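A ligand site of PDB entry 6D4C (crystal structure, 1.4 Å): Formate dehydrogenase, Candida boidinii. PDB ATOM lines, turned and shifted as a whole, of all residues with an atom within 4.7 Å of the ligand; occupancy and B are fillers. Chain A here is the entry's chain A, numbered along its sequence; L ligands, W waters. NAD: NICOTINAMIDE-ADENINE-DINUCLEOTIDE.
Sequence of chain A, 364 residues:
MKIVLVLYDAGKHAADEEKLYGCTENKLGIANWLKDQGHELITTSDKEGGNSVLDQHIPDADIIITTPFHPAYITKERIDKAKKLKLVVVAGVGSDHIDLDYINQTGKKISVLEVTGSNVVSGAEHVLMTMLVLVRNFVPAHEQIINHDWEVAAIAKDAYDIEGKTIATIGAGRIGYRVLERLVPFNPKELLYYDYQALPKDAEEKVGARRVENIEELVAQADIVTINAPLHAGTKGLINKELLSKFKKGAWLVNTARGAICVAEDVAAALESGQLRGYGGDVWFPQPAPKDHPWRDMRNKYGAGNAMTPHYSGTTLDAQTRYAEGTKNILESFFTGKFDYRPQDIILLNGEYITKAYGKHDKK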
ATOM      1  N   PHE A  69     -13.109  -3.874   0.650  1.00  0.00           N
ATOM      2  CA  PHE A  69     -12.143  -4.105   1.723  1.00  0.00           C
ATOM      3  C   PHE A  69     -11.266  -5.314   1.437  1.00  0.00           C
ATOM      4  O   PHE A  69     -10.218  -5.460   2.049  1.00  0.00           O
ATOM      5  CB  PHE A  69     -12.880  -4.241   3.074  1.00  0.00           C
ATOM      6  CG  PHE A  69     -14.055  -3.333   3.141  1.00  0.00           C
ATOM      7  CD1 PHE A  69     -13.889  -1.970   3.335  1.00  0.00           C
ATOM      8  CD2 PHE A  69     -15.315  -3.809   2.859  1.00  0.00           C
ATOM      9  CE1 PHE A  69     -14.959  -1.106   3.275  1.00  0.00           C
ATOM     10  CE2 PHE A  69     -16.372  -2.966   2.782  1.00  0.00           C
ATOM     11  CZ  PHE A  69     -16.218  -1.618   2.983  1.00  0.00           C
ATOM     12  N   VAL A  93     -18.868   0.804  -1.325  1.00  0.00           N
ATOM     13  CA  VAL A  93     -18.855   1.969  -2.208  1.00  0.00           C
ATOM     14  C   VAL A  93     -17.480   2.038  -2.872  1.00  0.00           C
ATOM     15  O   VAL A  93     -16.455   1.899  -2.199  1.00  0.00           O
ATOM     16  CB  VAL A  93     -19.141   3.244  -1.400  1.00  0.00           C
ATOM     17  CG1 VAL A  93     -18.887   4.485  -2.239  1.00  0.00           C
ATOM     18  CG2 VAL A  93     -20.583   3.230  -0.891  1.00  0.00           C
ATOM     19  N   GLY A  94     -17.474   2.240  -4.188  1.00  0.00           N
ATOM     20  CA  GLY A  94     -16.254   2.353  -4.991  1.00  0.00           C
ATOM     21  C   GLY A  94     -16.073   1.148  -5.879  1.00  0.00           C
ATOM     22  O   GLY A  94     -15.889   0.031  -5.377  1.00  0.00           O
ATOM     23  N   ASP A  96     -13.789   0.841  -8.542  1.00  0.00           N
ATOM     24  CA  ASP A  96     -12.527   0.961  -9.285  1.00  0.00           C
ATOM     25  C   ASP A  96     -11.739  -0.344  -9.348  1.00  0.00           C
ATOM     26  O   ASP A  96     -10.795  -0.439 -10.148  1.00  0.00           O
ATOM     27  CB  ASP A  96     -11.666   1.984  -8.555  1.00  0.00           C
ATOM     28  CG  ASP A  96     -11.628   1.721  -7.078  1.00  0.00           C
ATOM     29  OD1 ASP A  96     -12.566   2.194  -6.381  1.00  0.00           O
ATOM     30  OD2 ASP A  96     -10.685   1.029  -6.622  1.00  0.00           O
ATOM     31  N   ASN A 119     -22.052   3.616   3.476  1.00  0.00           N
ATOM     32  CA  ASN A 119     -20.997   3.798   4.467  1.00  0.00           C
ATOM     33  C   ASN A 119     -20.326   5.158   4.338  1.00  0.00           C
ATOM     34  O   ASN A 119     -19.174   5.335   4.777  1.00  0.00           O
ATOM     35  CB  ASN A 119     -19.979   2.676   4.379  1.00  0.00           C
ATOM     36  CG  ASN A 119     -19.381   2.553   3.008  1.00  0.00           C
ATOM     37  OD1 ASN A 119     -19.543   3.438   2.170  1.00  0.00           O
ATOM     38  ND2 ASN A 119     -18.693   1.445   2.749  1.00  0.00           N
ATOM     39  N   VAL A 120     -21.032   6.129   3.745  1.00  0.00           N
ATOM     40  CA  VAL A 120     -20.498   7.467   3.552  1.00  0.00           C
ATOM     41  C   VAL A 120     -20.354   8.195   4.890  1.00  0.00           C
ATOM     42  O   VAL A 120     -19.407   8.959   5.087  1.00  0.00           O
ATOM     43  CB  VAL A 120     -21.318   8.284   2.530  1.00  0.00           C
ATOM     44  CG1 VAL A 120     -21.312   7.544   1.183  1.00  0.00           C
ATOM     45  CG2 VAL A 120     -22.742   8.549   2.993  1.00  0.00           C
ATOM     46  N   ILE A 170     -10.730  17.366  -1.739  1.00  0.00           N
ATOM     47  CA  ILE A 170     -10.704  17.047  -3.162  1.00  0.00           C
ATOM     48  C   ILE A 170     -11.837  16.048  -3.359  1.00  0.00           C
ATOM     49  O   ILE A 170     -11.737  14.876  -2.977  1.00  0.00           O
ATOM     50  CB  ILE A 170      -9.346  16.479  -3.572  1.00  0.00           C
ATOM     51  CG1 ILE A 170      -8.268  17.571  -3.462  1.00  0.00           C
ATOM     52  CG2 ILE A 170      -9.385  15.898  -4.971  1.00  0.00           C
ATOM     53  CD1 ILE A 170      -6.849  17.020  -3.438  1.00  0.00           C
ATOM     54  N   GLY A 171     -12.947  16.538  -3.892  1.00  0.00           N
ATOM     55  CA  GLY A 171     -14.172  15.778  -4.012  1.00  0.00           C
ATOM     56  C   GLY A 171     -15.102  16.237  -2.923  1.00  0.00           C
ATOM     57  O   GLY A 171     -14.768  16.205  -1.742  1.00  0.00           O
ATOM     58  N   ALA A 172     -16.259  16.745  -3.303  1.00  0.00           N
ATOM     59  CA  ALA A 172     -17.258  17.237  -2.361  1.00  0.00           C
ATOM     60  C   ALA A 172     -18.576  16.548  -2.625  1.00  0.00           C
ATOM     61  O   ALA A 172     -19.614  17.195  -2.799  1.00  0.00           O
ATOM     62  CB  ALA A 172     -17.417  18.762  -2.409  1.00  0.00           C
ATOM     63  N   GLY A 173     -18.536  15.221  -2.716  1.00  0.00           N
ATOM     64  CA  GLY A 173     -19.733  14.424  -2.858  1.00  0.00           C
ATOM     65  C   GLY A 173     -20.259  13.958  -1.522  1.00  0.00           C
ATOM     66  O   GLY A 173     -20.222  14.721  -0.539  1.00  0.00           O
ATOM     67  N   ARG A 174     -20.740  12.718  -1.442  1.00  0.00           N
ATOM     68  CA  ARG A 174     -21.404  12.266  -0.213  1.00  0.00           C
ATOM     69  C   ARG A 174     -20.459  12.310   0.967  1.00  0.00           C
ATOM     70  O   ARG A 174     -20.822  12.823   2.046  1.00  0.00           O
ATOM     71  CB  ARG A 174     -22.022  10.885  -0.403  1.00  0.00           C
ATOM     72  CG  ARG A 174     -23.227  10.950  -1.320  1.00  0.00           C
ATOM     73  CD  ARG A 174     -23.652   9.574  -1.754  1.00  0.00           C
ATOM     74  NE  ARG A 174     -24.781   9.612  -2.702  1.00  0.00           N
ATOM     75  CZ  ARG A 174     -24.662   9.818  -4.005  1.00  0.00           C
ATOM     76  NH1 ARG A 174     -23.487  10.011  -4.587  1.00  0.00           N
ATOM     77  NH2 ARG A 174     -25.757   9.835  -4.760  1.00  0.00           N
ATOM     78  N   ILE A 175     -19.246  11.795   0.802  1.00  0.00           N
ATOM     79  CA  ILE A 175     -18.295  11.790   1.923  1.00  0.00           C
ATOM     80  C   ILE A 175     -17.703  13.186   2.127  1.00  0.00           C
ATOM     81  O   ILE A 175     -17.666  13.697   3.241  1.00  0.00           O
ATOM     82  CB  ILE A 175     -17.208  10.713   1.763  1.00  0.00           C
ATOM     83  CG1 ILE A 175     -17.867   9.329   1.808  1.00  0.00           C
ATOM     84  CG2 ILE A 175     -16.166  10.875   2.893  1.00  0.00           C
ATOM     85  CD1 ILE A 175     -16.994   8.172   1.472  1.00  0.00           C
ATOM     86  N   GLY A 176     -17.186  13.784   1.062  1.00  0.00           N
ATOM     87  CA  GLY A 176     -16.564  15.093   1.203  1.00  0.00           C
ATOM     88  C   GLY A 176     -17.486  16.111   1.863  1.00  0.00           C
ATOM     89  O   GLY A 176     -17.074  16.868   2.741  1.00  0.00           O
ATOM     90  N   TYR A 194     -12.572  21.374  -4.004  1.00  0.00           N
ATOM     91  CA  TYR A 194     -12.325  21.286  -5.429  1.00  0.00           C
ATOM     92  C   TYR A 194     -13.106  20.080  -5.943  1.00  0.00           C
ATOM     93  O   TYR A 194     -12.929  18.957  -5.438  1.00  0.00           O
ATOM     94  CB  TYR A 194     -10.833  21.079  -5.681  1.00  0.00           C
ATOM     95  CG  TYR A 194     -10.437  20.663  -7.082  1.00  0.00           C
ATOM     96  CD1 TYR A 194     -10.390  21.594  -8.111  1.00  0.00           C
ATOM     97  CD2 TYR A 194     -10.074  19.359  -7.374  1.00  0.00           C
ATOM     98  CE1 TYR A 194      -9.996  21.219  -9.406  1.00  0.00           C
ATOM     99  CE2 TYR A 194      -9.663  18.973  -8.659  1.00  0.00           C
ATOM    100  CZ  TYR A 194      -9.636  19.918  -9.668  1.00  0.00           C
ATOM    101  OH  TYR A 194      -9.232  19.569 -10.951  1.00  0.00           O
ATOM    102  N   ASP A 195     -13.921  20.303  -6.959  1.00  0.00           N
ATOM    103  CA  ASP A 195     -14.748  19.269  -7.561  1.00  0.00           C
ATOM    104  C   ASP A 195     -15.256  19.849  -8.859  1.00  0.00           C
ATOM    105  O   ASP A 195     -15.638  21.019  -8.896  1.00  0.00           O
ATOM    106  CB  ASP A 195     -15.933  18.957  -6.628  1.00  0.00           C
ATOM    107  CG  ASP A 195     -16.621  17.635  -6.945  1.00  0.00           C
ATOM    108  OD1 ASP A 195     -16.702  17.248  -8.122  1.00  0.00           O
ATOM    109  OD2 ASP A 195     -17.073  16.937  -5.990  1.00  0.00           O
ATOM    110  N   TYR A 196     -15.264  19.050  -9.917  1.00  0.00           N
ATOM    111  CA  TYR A 196     -15.890  19.521 -11.158  1.00  0.00           C
ATOM    112  C   TYR A 196     -17.402  19.662 -11.017  1.00  0.00           C
ATOM    113  O   TYR A 196     -18.021  20.374 -11.823  1.00  0.00           O
ATOM    114  CB  TYR A 196     -15.494  18.628 -12.330  1.00  0.00           C
ATOM    115  CG  TYR A 196     -15.857  17.153 -12.241  1.00  0.00           C
ATOM    116  CD1 TYR A 196     -17.164  16.731 -12.414  1.00  0.00           C
ATOM    117  CD2 TYR A 196     -14.869  16.198 -12.081  1.00  0.00           C
ATOM    118  CE1 TYR A 196     -17.493  15.375 -12.374  1.00  0.00           C
ATOM    119  CE2 TYR A 196     -15.182  14.849 -12.054  1.00  0.00           C
ATOM    120  CZ  TYR A 196     -16.491  14.439 -12.208  1.00  0.00           C
ATOM    121  OH  TYR A 196     -16.740  13.079 -12.171  1.00  0.00           O
ATOM    122  N   GLN A 197     -17.996  19.014 -10.021  1.00  0.00           N
ATOM    123  CA  GLN A 197     -19.397  19.171  -9.674  1.00  0.00           C
ATOM    124  C   GLN A 197     -19.492  20.174  -8.541  1.00  0.00           C
ATOM    125  O   GLN A 197     -19.010  19.925  -7.437  1.00  0.00           O
ATOM    126  CB  GLN A 197     -19.984  17.831  -9.237  1.00  0.00           C
ATOM    127  CG  GLN A 197     -21.416  17.904  -8.739  1.00  0.00           C
ATOM    128  CD  GLN A 197     -22.362  18.484  -9.800  1.00  0.00           C
ATOM    129  OE1 GLN A 197     -22.429  17.988 -10.939  1.00  0.00           O
ATOM    130  NE2 GLN A 197     -23.068  19.556  -9.443  1.00  0.00           N
ATOM    131  N   ASN A 228     -11.539  12.748  -1.265  1.00  0.00           N
ATOM    132  CA  ASN A 228     -12.857  12.146  -1.211  1.00  0.00           C
ATOM    133  C   ASN A 228     -13.456  12.061  -2.615  1.00  0.00           C
ATOM    134  O   ASN A 228     -14.616  12.407  -2.836  1.00  0.00           O
ATOM    135  CB  ASN A 228     -13.782  12.908  -0.257  1.00  0.00           C
ATOM    136  CG  ASN A 228     -13.262  12.874   1.142  1.00  0.00           C
ATOM    137  OD1 ASN A 228     -13.271  11.807   1.767  1.00  0.00           O
ATOM    138  ND2 ASN A 228     -12.768  13.999   1.635  1.00  0.00           N
ATOM    139  N   ALA A 229     -12.669  11.623  -3.578  1.00  0.00           N
ATOM    140  CA  ALA A 229     -13.161  11.390  -4.912  1.00  0.00           C
ATOM    141  C   ALA A 229     -12.957   9.920  -5.248  1.00  0.00           C
ATOM    142  O   ALA A 229     -12.138   9.233  -4.632  1.00  0.00           O
ATOM    143  CB  ALA A 229     -12.398  12.275  -5.905  1.00  0.00           C
ATOM    144  N   PRO A 230     -13.723   9.381  -6.194  1.00  0.00           N
ATOM    145  CA  PRO A 230     -13.509   8.000  -6.595  1.00  0.00           C
ATOM    146  C   PRO A 230     -12.209   7.889  -7.380  1.00  0.00           C
ATOM    147  O   PRO A 230     -11.644   8.884  -7.853  1.00  0.00           O
ATOM    148  CB  PRO A 230     -14.706   7.695  -7.513  1.00  0.00           C
ATOM    149  CG  PRO A 230     -15.645   8.855  -7.322  1.00  0.00           C
ATOM    150  CD  PRO A 230     -14.743  10.003  -7.047  1.00  0.00           C
ATOM    151  N   LEU A 231     -11.739   6.650  -7.490  1.00  0.00           N
ATOM    152  CA  LEU A 231     -10.580   6.328  -8.321  1.00  0.00           C
ATOM    153  C   LEU A 231     -11.054   6.069  -9.731  1.00  0.00           C
ATOM    154  O   LEU A 231     -11.881   5.182  -9.984  1.00  0.00           O
ATOM    155  CB  LEU A 231      -9.862   5.087  -7.811  1.00  0.00           C
ATOM    156  CG  LEU A 231      -8.659   4.593  -8.645  1.00  0.00           C
ATOM    157  CD1 LEU A 231      -7.572   5.654  -8.753  1.00  0.00           C
ATOM    158  CD2 LEU A 231      -8.093   3.321  -8.041  1.00  0.00           C
ATOM    159  N   HIS A 232     -10.540   6.869 -10.657  1.00  0.00           N
ATOM    160  CA  HIS A 232     -10.794   6.695 -12.071  1.00  0.00           C
ATOM    161  C   HIS A 232      -9.610   7.314 -12.797  1.00  0.00           C
ATOM    162  O   HIS A 232      -8.672   7.785 -12.163  1.00  0.00           O
ATOM    163  CB  HIS A 232     -12.131   7.326 -12.478  1.00  0.00           C
ATOM    164  CG  HIS A 232     -12.223   8.805 -12.207  1.00  0.00           C
ATOM    165  ND1 HIS A 232     -11.833   9.745 -13.137  1.00  0.00           N
ATOM    166  CD2 HIS A 232     -12.658   9.501 -11.125  1.00  0.00           C
ATOM    167  CE1 HIS A 232     -12.041  10.961 -12.652  1.00  0.00           C
ATOM    168  NE2 HIS A 232     -12.550  10.837 -11.437  1.00  0.00           N
ATOM    169  N   GLY A 234      -8.977  10.048 -14.176  1.00  0.00           N
ATOM    170  CA  GLY A 234      -8.653  11.421 -13.818  1.00  0.00           C
ATOM    171  C   GLY A 234      -8.088  11.619 -12.420  1.00  0.00           C
ATOM    172  O   GLY A 234      -7.565  12.698 -12.112  1.00  0.00           O
ATOM    173  N   THR A 235      -8.189  10.613 -11.554  1.00  0.00           N
ATOM    174  CA  THR A 235      -7.647  10.708 -10.205  1.00  0.00           C
ATOM    175  C   THR A 235      -6.514   9.715  -9.939  1.00  0.00           C
ATOM    176  O   THR A 235      -5.843   9.844  -8.918  1.00  0.00           O
ATOM    177  CB  THR A 235      -8.748  10.500  -9.141  1.00  0.00           C
ATOM    178  OG1 THR A 235      -9.401   9.238  -9.363  1.00  0.00           O
ATOM    179  CG2 THR A 235      -9.747  11.615  -9.206  1.00  0.00           C
ATOM    180  N   THR A 256      -9.069   8.487   2.769  1.00  0.00           N
ATOM    181  CA  THR A 256      -9.949   7.353   2.935  1.00  0.00           C
ATOM    182  C   THR A 256     -10.667   7.014   1.642  1.00  0.00           C
ATOM    183  O   THR A 256     -11.654   6.279   1.660  1.00  0.00           O
ATOM    184  CB  THR A 256     -10.986   7.670   4.009  1.00  0.00           C
ATOM    185  OG1 THR A 256     -11.732   8.833   3.608  1.00  0.00           O
ATOM    186  CG2 THR A 256     -10.331   7.931   5.348  1.00  0.00           C
ATOM    187  N   ALA A 257     -10.224   7.579   0.524  1.00  0.00           N
ATOM    188  CA  ALA A 257     -10.916   7.377  -0.740  1.00  0.00           C
ATOM    189  C   ALA A 257     -10.404   6.103  -1.391  1.00  0.00           C
ATOM    190  O   ALA A 257     -10.978   5.026  -1.214  1.00  0.00           O
ATOM    191  CB  ALA A 257     -10.725   8.611  -1.621  1.00  0.00           C
ATOM    192  N   ARG A 258      -9.268   6.203  -2.085  1.00  0.00           N
ATOM    193  CA  ARG A 258      -8.588   5.054  -2.670  1.00  0.00           C
ATOM    194  C   ARG A 258      -7.089   5.309  -2.652  1.00  0.00           C
ATOM    195  O   ARG A 258      -6.642   6.417  -2.914  1.00  0.00           O
ATOM    196  CB  ARG A 258      -9.027   4.765  -4.105  1.00  0.00           C
ATOM    197  CG  ARG A 258     -10.428   4.195  -4.226  1.00  0.00           C
ATOM    198  CD  ARG A 258     -10.494   2.843  -3.525  1.00  0.00           C
ATOM    199  NE  ARG A 258     -11.775   2.150  -3.701  1.00  0.00           N
ATOM    200  CZ  ARG A 258     -12.720   2.037  -2.770  1.00  0.00           C
ATOM    201  NH1 ARG A 258     -12.617   2.642  -1.578  1.00  0.00           N
ATOM    202  NH2 ARG A 258     -13.812   1.323  -3.072  1.00  0.00           N
ATOM    203  N   ASP A 282      -7.182   4.703   5.446  1.00  0.00           N
ATOM    204  CA  ASP A 282      -7.413   3.262   5.527  1.00  0.00           C
ATOM    205  C   ASP A 282      -7.252   2.525   4.209  1.00  0.00           C
ATOM    206  O   ASP A 282      -7.337   1.305   4.187  1.00  0.00           O
ATOM    207  CB  ASP A 282      -8.803   2.999   6.151  1.00  0.00           C
ATOM    208  CG  ASP A 282      -9.960   3.493   5.312  1.00  0.00           C
ATOM    209  OD1 ASP A 282      -9.792   4.526   4.623  1.00  0.00           O
ATOM    210  OD2 ASP A 282     -11.036   2.849   5.378  1.00  0.00           O
ATOM    211  N   VAL A 283      -6.995   3.229   3.113  1.00  0.00           N
ATOM    212  CA  VAL A 283      -7.017   2.635   1.776  1.00  0.00           C
ATOM    213  C   VAL A 283      -5.626   2.592   1.174  1.00  0.00           C
ATOM    214  O   VAL A 283      -4.813   3.523   1.344  1.00  0.00           O
ATOM    215  CB  VAL A 283      -8.012   3.374   0.854  1.00  0.00           C
ATOM    216  CG1 VAL A 283      -9.410   3.179   1.370  1.00  0.00           C
ATOM    217  CG2 VAL A 283      -7.675   4.882   0.756  1.00  0.00           C
ATOM    218  N   HIS A 311      -7.966  -1.391   5.506  1.00  0.00           N
ATOM    219  CA  HIS A 311      -9.180  -0.841   4.905  1.00  0.00           C
ATOM    220  C   HIS A 311     -10.406  -1.332   5.635  1.00  0.00           C
ATOM    221  O   HIS A 311     -10.951  -2.401   5.334  1.00  0.00           O
ATOM    222  CB  HIS A 311      -9.243  -1.166   3.421  1.00  0.00           C
ATOM    223  CG  HIS A 311     -10.398  -0.495   2.737  1.00  0.00           C
ATOM    224  ND1 HIS A 311     -10.753  -0.798   1.454  1.00  0.00           N
ATOM    225  CD2 HIS A 311     -11.264   0.452   3.156  1.00  0.00           C
ATOM    226  CE1 HIS A 311     -11.805  -0.080   1.110  1.00  0.00           C
ATOM    227  NE2 HIS A 311     -12.143   0.685   2.131  1.00  0.00           N
ATOM    228  N   SER A 313     -12.799   1.414   7.281  1.00  0.00           N
ATOM    229  CA  SER A 313     -13.700   2.456   7.769  1.00  0.00           C
ATOM    230  C   SER A 313     -15.114   2.239   7.261  1.00  0.00           C
ATOM    231  O   SER A 313     -16.087   2.504   7.972  1.00  0.00           O
ATOM    232  CB  SER A 313     -13.196   3.859   7.420  1.00  0.00           C
ATOM    233  OG  SER A 313     -13.378   4.195   6.059  1.00  0.00           O
ATOM    234  N   GLY A 314     -15.246   1.759   6.035  1.00  0.00           N
ATOM    235  CA  GLY A 314     -16.537   1.482   5.432  1.00  0.00           C
ATOM    236  C   GLY A 314     -17.116   0.133   5.780  1.00  0.00           C
ATOM    237  O   GLY A 314     -18.165  -0.222   5.232  1.00  0.00           O
ATOM    238  N   ALA A 357     -19.679  10.644 -11.554  1.00  0.00           N
ATOM    239  CA  ALA A 357     -18.634  10.911 -10.585  1.00  0.00           C
ATOM    240  C   ALA A 357     -17.302  10.252 -10.905  1.00  0.00           C
ATOM    241  O   ALA A 357     -16.334  10.440 -10.147  1.00  0.00           O
ATOM    242  CB  ALA A 357     -19.098  10.402  -9.219  1.00  0.00           C
ATOM    243  N   TYR A 358     -17.233   9.475 -11.981  1.00  0.00           N
ATOM    244  CA  TYR A 358     -16.026   8.778 -12.405  1.00  0.00           C
ATOM    245  C   TYR A 358     -15.407   9.471 -13.611  1.00  0.00           C
ATOM    246  O   TYR A 358     -14.928   8.815 -14.532  1.00  0.00           O
ATOM    247  CB  TYR A 358     -16.316   7.286 -12.678  1.00  0.00           C
ATOM    248  CG  TYR A 358     -16.374   6.482 -11.390  1.00  0.00           C
ATOM    249  CD1 TYR A 358     -17.412   6.674 -10.483  1.00  0.00           C
ATOM    250  CD2 TYR A 358     -15.404   5.548 -11.076  1.00  0.00           C
ATOM    251  CE1 TYR A 358     -17.466   5.944  -9.299  1.00  0.00           C
ATOM    252  CE2 TYR A 358     -15.451   4.833  -9.906  1.00  0.00           C
ATOM    253  CZ  TYR A 358     -16.481   5.030  -9.033  1.00  0.00           C
ATOM    254  OH  TYR A 358     -16.468   4.321  -7.858  1.00  0.00           O
HETATM  255  PA  NAD L   1     -19.689  10.492  -4.473  1.00  0.00           P
HETATM  256  O1A NAD L   1     -19.860   9.912  -5.854  1.00  0.00           O
HETATM  257  O2A NAD L   1     -20.877  10.932  -3.720  1.00  0.00           O
HETATM  258  O5B NAD L   1     -18.729  11.748  -4.513  1.00  0.00           O
HETATM  259  C5B NAD L   1     -17.522  11.719  -5.276  1.00  0.00           C
HETATM  260  C4B NAD L   1     -17.184  13.194  -5.667  1.00  0.00           C
HETATM  261  O4B NAD L   1     -15.952  13.141  -6.204  1.00  0.00           O
HETATM  262  C3B NAD L   1     -18.152  13.691  -6.732  1.00  0.00           C
HETATM  263  O3B NAD L   1     -18.731  14.901  -6.390  1.00  0.00           O
HETATM  264  C2B NAD L   1     -17.184  13.779  -7.930  1.00  0.00           C
HETATM  265  O2B NAD L   1     -17.632  14.840  -8.853  1.00  0.00           O
HETATM  266  C1B NAD L   1     -15.982  14.067  -7.410  1.00  0.00           C
HETATM  267  N9A NAD L   1     -14.821  13.868  -8.249  1.00  0.00           N
HETATM  268  C8A NAD L   1     -14.600  12.969  -9.233  1.00  0.00           C
HETATM  269  N7A NAD L   1     -13.387  13.193  -9.771  1.00  0.00           N
HETATM  270  C5A NAD L   1     -12.848  14.259  -9.171  1.00  0.00           C
HETATM  271  C6A NAD L   1     -11.674  14.913  -9.384  1.00  0.00           C
HETATM  272  N6A NAD L   1     -10.680  14.607 -10.311  1.00  0.00           N
HETATM  273  N1A NAD L   1     -11.378  15.921  -8.621  1.00  0.00           N
HETATM  274  C2A NAD L   1     -12.231  16.356  -7.671  1.00  0.00           C
HETATM  275  N3A NAD L   1     -13.425  15.743  -7.470  1.00  0.00           N
HETATM  276  C4A NAD L   1     -13.737  14.684  -8.220  1.00  0.00           C
HETATM  277  O3  NAD L   1     -18.875   9.389  -3.686  1.00  0.00           O
HETATM  278  PN  NAD L   1     -18.627   9.240  -2.061  1.00  0.00           P
HETATM  279  O1N NAD L   1     -18.301  10.593  -1.536  1.00  0.00           O
HETATM  280  O2N NAD L   1     -19.711   8.465  -1.435  1.00  0.00           O
HETATM  281  O5D NAD L   1     -17.347   8.328  -2.058  1.00  0.00           O
HETATM  282  C5D NAD L   1     -16.150   8.753  -2.714  1.00  0.00           C
HETATM  283  C4D NAD L   1     -15.103   7.624  -2.735  1.00  0.00           C
HETATM  284  O4D NAD L   1     -14.733   7.328  -1.468  1.00  0.00           O
HETATM  285  C3D NAD L   1     -15.747   6.345  -3.317  1.00  0.00           C
HETATM  286  O3D NAD L   1     -15.775   6.333  -4.717  1.00  0.00           O
HETATM  287  C2D NAD L   1     -14.845   5.325  -2.635  1.00  0.00           C
HETATM  288  O2D NAD L   1     -13.680   5.116  -3.546  1.00  0.00           O
HETATM  289  C1D NAD L   1     -14.363   5.838  -1.456  1.00  0.00           C
HETATM  290  N1N NAD L   1     -14.918   5.262  -0.272  1.00  0.00           N
HETATM  291  C2N NAD L   1     -14.107   4.667   0.684  1.00  0.00           C
HETATM  292  C3N NAD L   1     -14.702   4.099   1.810  1.00  0.00           C
HETATM  293  C7N NAD L   1     -13.805   3.430   2.835  1.00  0.00           C
HETATM  294  O7N NAD L   1     -14.189   2.459   3.455  1.00  0.00           O
HETATM  295  N7N NAD L   1     -12.488   3.941   2.943  1.00  0.00           N
HETATM  296  C4N NAD L   1     -16.062   4.061   1.988  1.00  0.00           C
HETATM  297  C5N NAD L   1     -16.894   4.657   1.049  1.00  0.00           C
HETATM  298  C6N NAD L   1     -16.298   5.247  -0.084  1.00  0.00           C
HETATM  299  O   HOH W   1     -17.065  12.970  -1.689  1.00  0.00           O
HETATM  300  O   HOH W   2     -18.042   5.316  -5.955  1.00  0.00           O
HETATM  301  O   HOH W   3     -22.550  13.081  -4.483  1.00  0.00           O
HETATM  302  O   HOH W   4     -19.978   7.285  -6.317  1.00  0.00           O
HETATM  303  O   HOH W   5     -13.714   4.652  -6.405  1.00  0.00           O
HETATM  304  O   HOH W   6     -20.096  14.065 -10.085  1.00  0.00           O
HETATM  305  O   HOH W   7     -21.680   6.621  -1.961  1.00  0.00           O
HETATM  306  O   HOH W   8     -22.144  10.589  -7.148  1.00  0.00           O
HETATM  307  O   HOH W   9     -21.414  15.165  -6.065  1.00  0.00           O
HETATM  308  O   HOH W  10     -12.340  18.197 -10.742  1.00  0.00           O
HETATM  309  O   HOH W  11     -13.371   9.123   1.019  1.00  0.00           O
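The side-chain carboxylate (OD2) of Asp 195 sits at hydrogen-bond distance from an oxygen (O3B) of the ligand (2.7 Å).
N of Ile 175 lies within hydrogen-bond range of O1N of the ligand, at 2.8 Å.
A nitrogen (N7N) of the ligand sits at hydrogen-bond distance from the backbone carbonyl oxygen of Thr 256 (2.8 Å).
The backbone NH (N) of Gly 314 is in hydrogen-bond range of an oxygen (O7N) of the ligand, at 2.9 Å.
N of Arg 174 lies within hydrogen-bond range of O2A of the ligand (2.9 Å).
The guanidinium group of Arg 174 is in salt-bridge range of an oxygen (O2A) of the ligand, at 2.9 Å.
N7A of the ligand is in hydrogen-bond range of NE2 of His 232, at 3.0 Å.
O7N of the ligand lies within hydrogen-bond range of NE2 of His 311 (3.0 Å).
The side-chain carboxylate (OD2) of Asp 282 is in hydrogen-bond range of a nitrogen (N7N) of the ligand (3.0 Å).
O7N of the ligand is in hydrogen-bond range of OG of Ser 313 (3.2 Å).
The guanidinium group (NH1) of Arg 258 lies close to an oxygen (O2D) of the ligand (3.3 Å).
The backbone NH (N) of Gln 197 sits at hydrogen-bond distance from the side-chain carboxylate (OD1) of Asp 195 (2.9 Å).
The backbone NH (N) of His 232 is in hydrogen-bond range of the side-chain hydroxyl (OG1) of Thr 235, 2.9 Å away.
The side-chain carboxylate of Asp 282 sits at hydrogen-bond distance from the side-chain hydroxyl of Ser 313 (2.8 Å).
The backbone carbonyl oxygen (O) of Pro 230 lies within hydrogen-bond range of the side-chain hydroxyl (OG1) of Thr 235 (2.7 Å).
NH2 of Arg 258 is in hydrogen-bond range of O of Val 93 (2.8 Å).
The guanidinium group (NH2) of Arg 258 lies close to the backbone carbonyl oxygen (O) of Gly 94 (3.4 Å).
OD1 of Asp 96 is in salt-bridge range of NE of Arg 258.
The backbone NH (N) of Ala 229 sits at hydrogen-bond distance from the backbone carbonyl oxygen (O) of Ile 170.
Residues that only touch the ligand: Phe 69, Val 93, Asn 119, Val 120, Ile 170, Gly 171, Gly 173, Tyr 194, Tyr 196, Gln 197, Asn 228, Ala 229, Pro 230, Thr 235, Ala 257, Val 283, Ala 357 and Tyr 358.
Hydrophobic or aromatic side chains that line the ligand: Phe 69, Val 93, Val 120, Ile 170, Ile 175, Tyr 194, Tyr 196, Ala 229, Pro 230, His 232, Val 283, His 311 and Ala 357.
Within 4 Å of the ligand: Phe 69, Val 93, Asn 119, Val 120, Ile 170, Gly 171, Gly 173, Arg 174, Ile 175, Tyr 194, Asp 195, Tyr 196, Gln 197, Asn 228, Ala 229, Pro 230, His 232, Thr 235, Thr 256, Ala 257, Arg 258, Asp 282, Val 283, His 311, Ser 313, Gly 314, Ala 357 and Tyr 358.
Water W1 lies within hydrogen-bond range of an oxygen (O1N) of the ligand, the backbone carbonyl oxygen of Asn 228, the backbone NH of Gly 176 and the backbone NH of Gly 173.
Water W8 bridges an oxygen (O1A) of the ligand and the guanidinium group of Arg 174.
Water W2 lies within hydrogen-bond range of the side-chain hydroxyl (OH) of Tyr 358 (2.7 Å) and an oxygen (O3D) of the ligand (2.8 Å).
Water W3 lies within hydrogen-bond range of O2A of the ligand (2.8 Å) and NH1 of Arg 174 (3.2 Å).
Water W5 lies within hydrogen-bond range of the side-chain carboxylate (OD1) of Asp 96 (2.7 Å), an oxygen (O2D) of the ligand (2.9 Å), the backbone NH (N) of Leu 231 (3.0 Å) and the side-chain hydroxyl (OH) of Tyr 358 (3.1 Å).
Water W10 lies within hydrogen-bond range of N of Tyr 196, N1A of the ligand and OH of Tyr 194.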
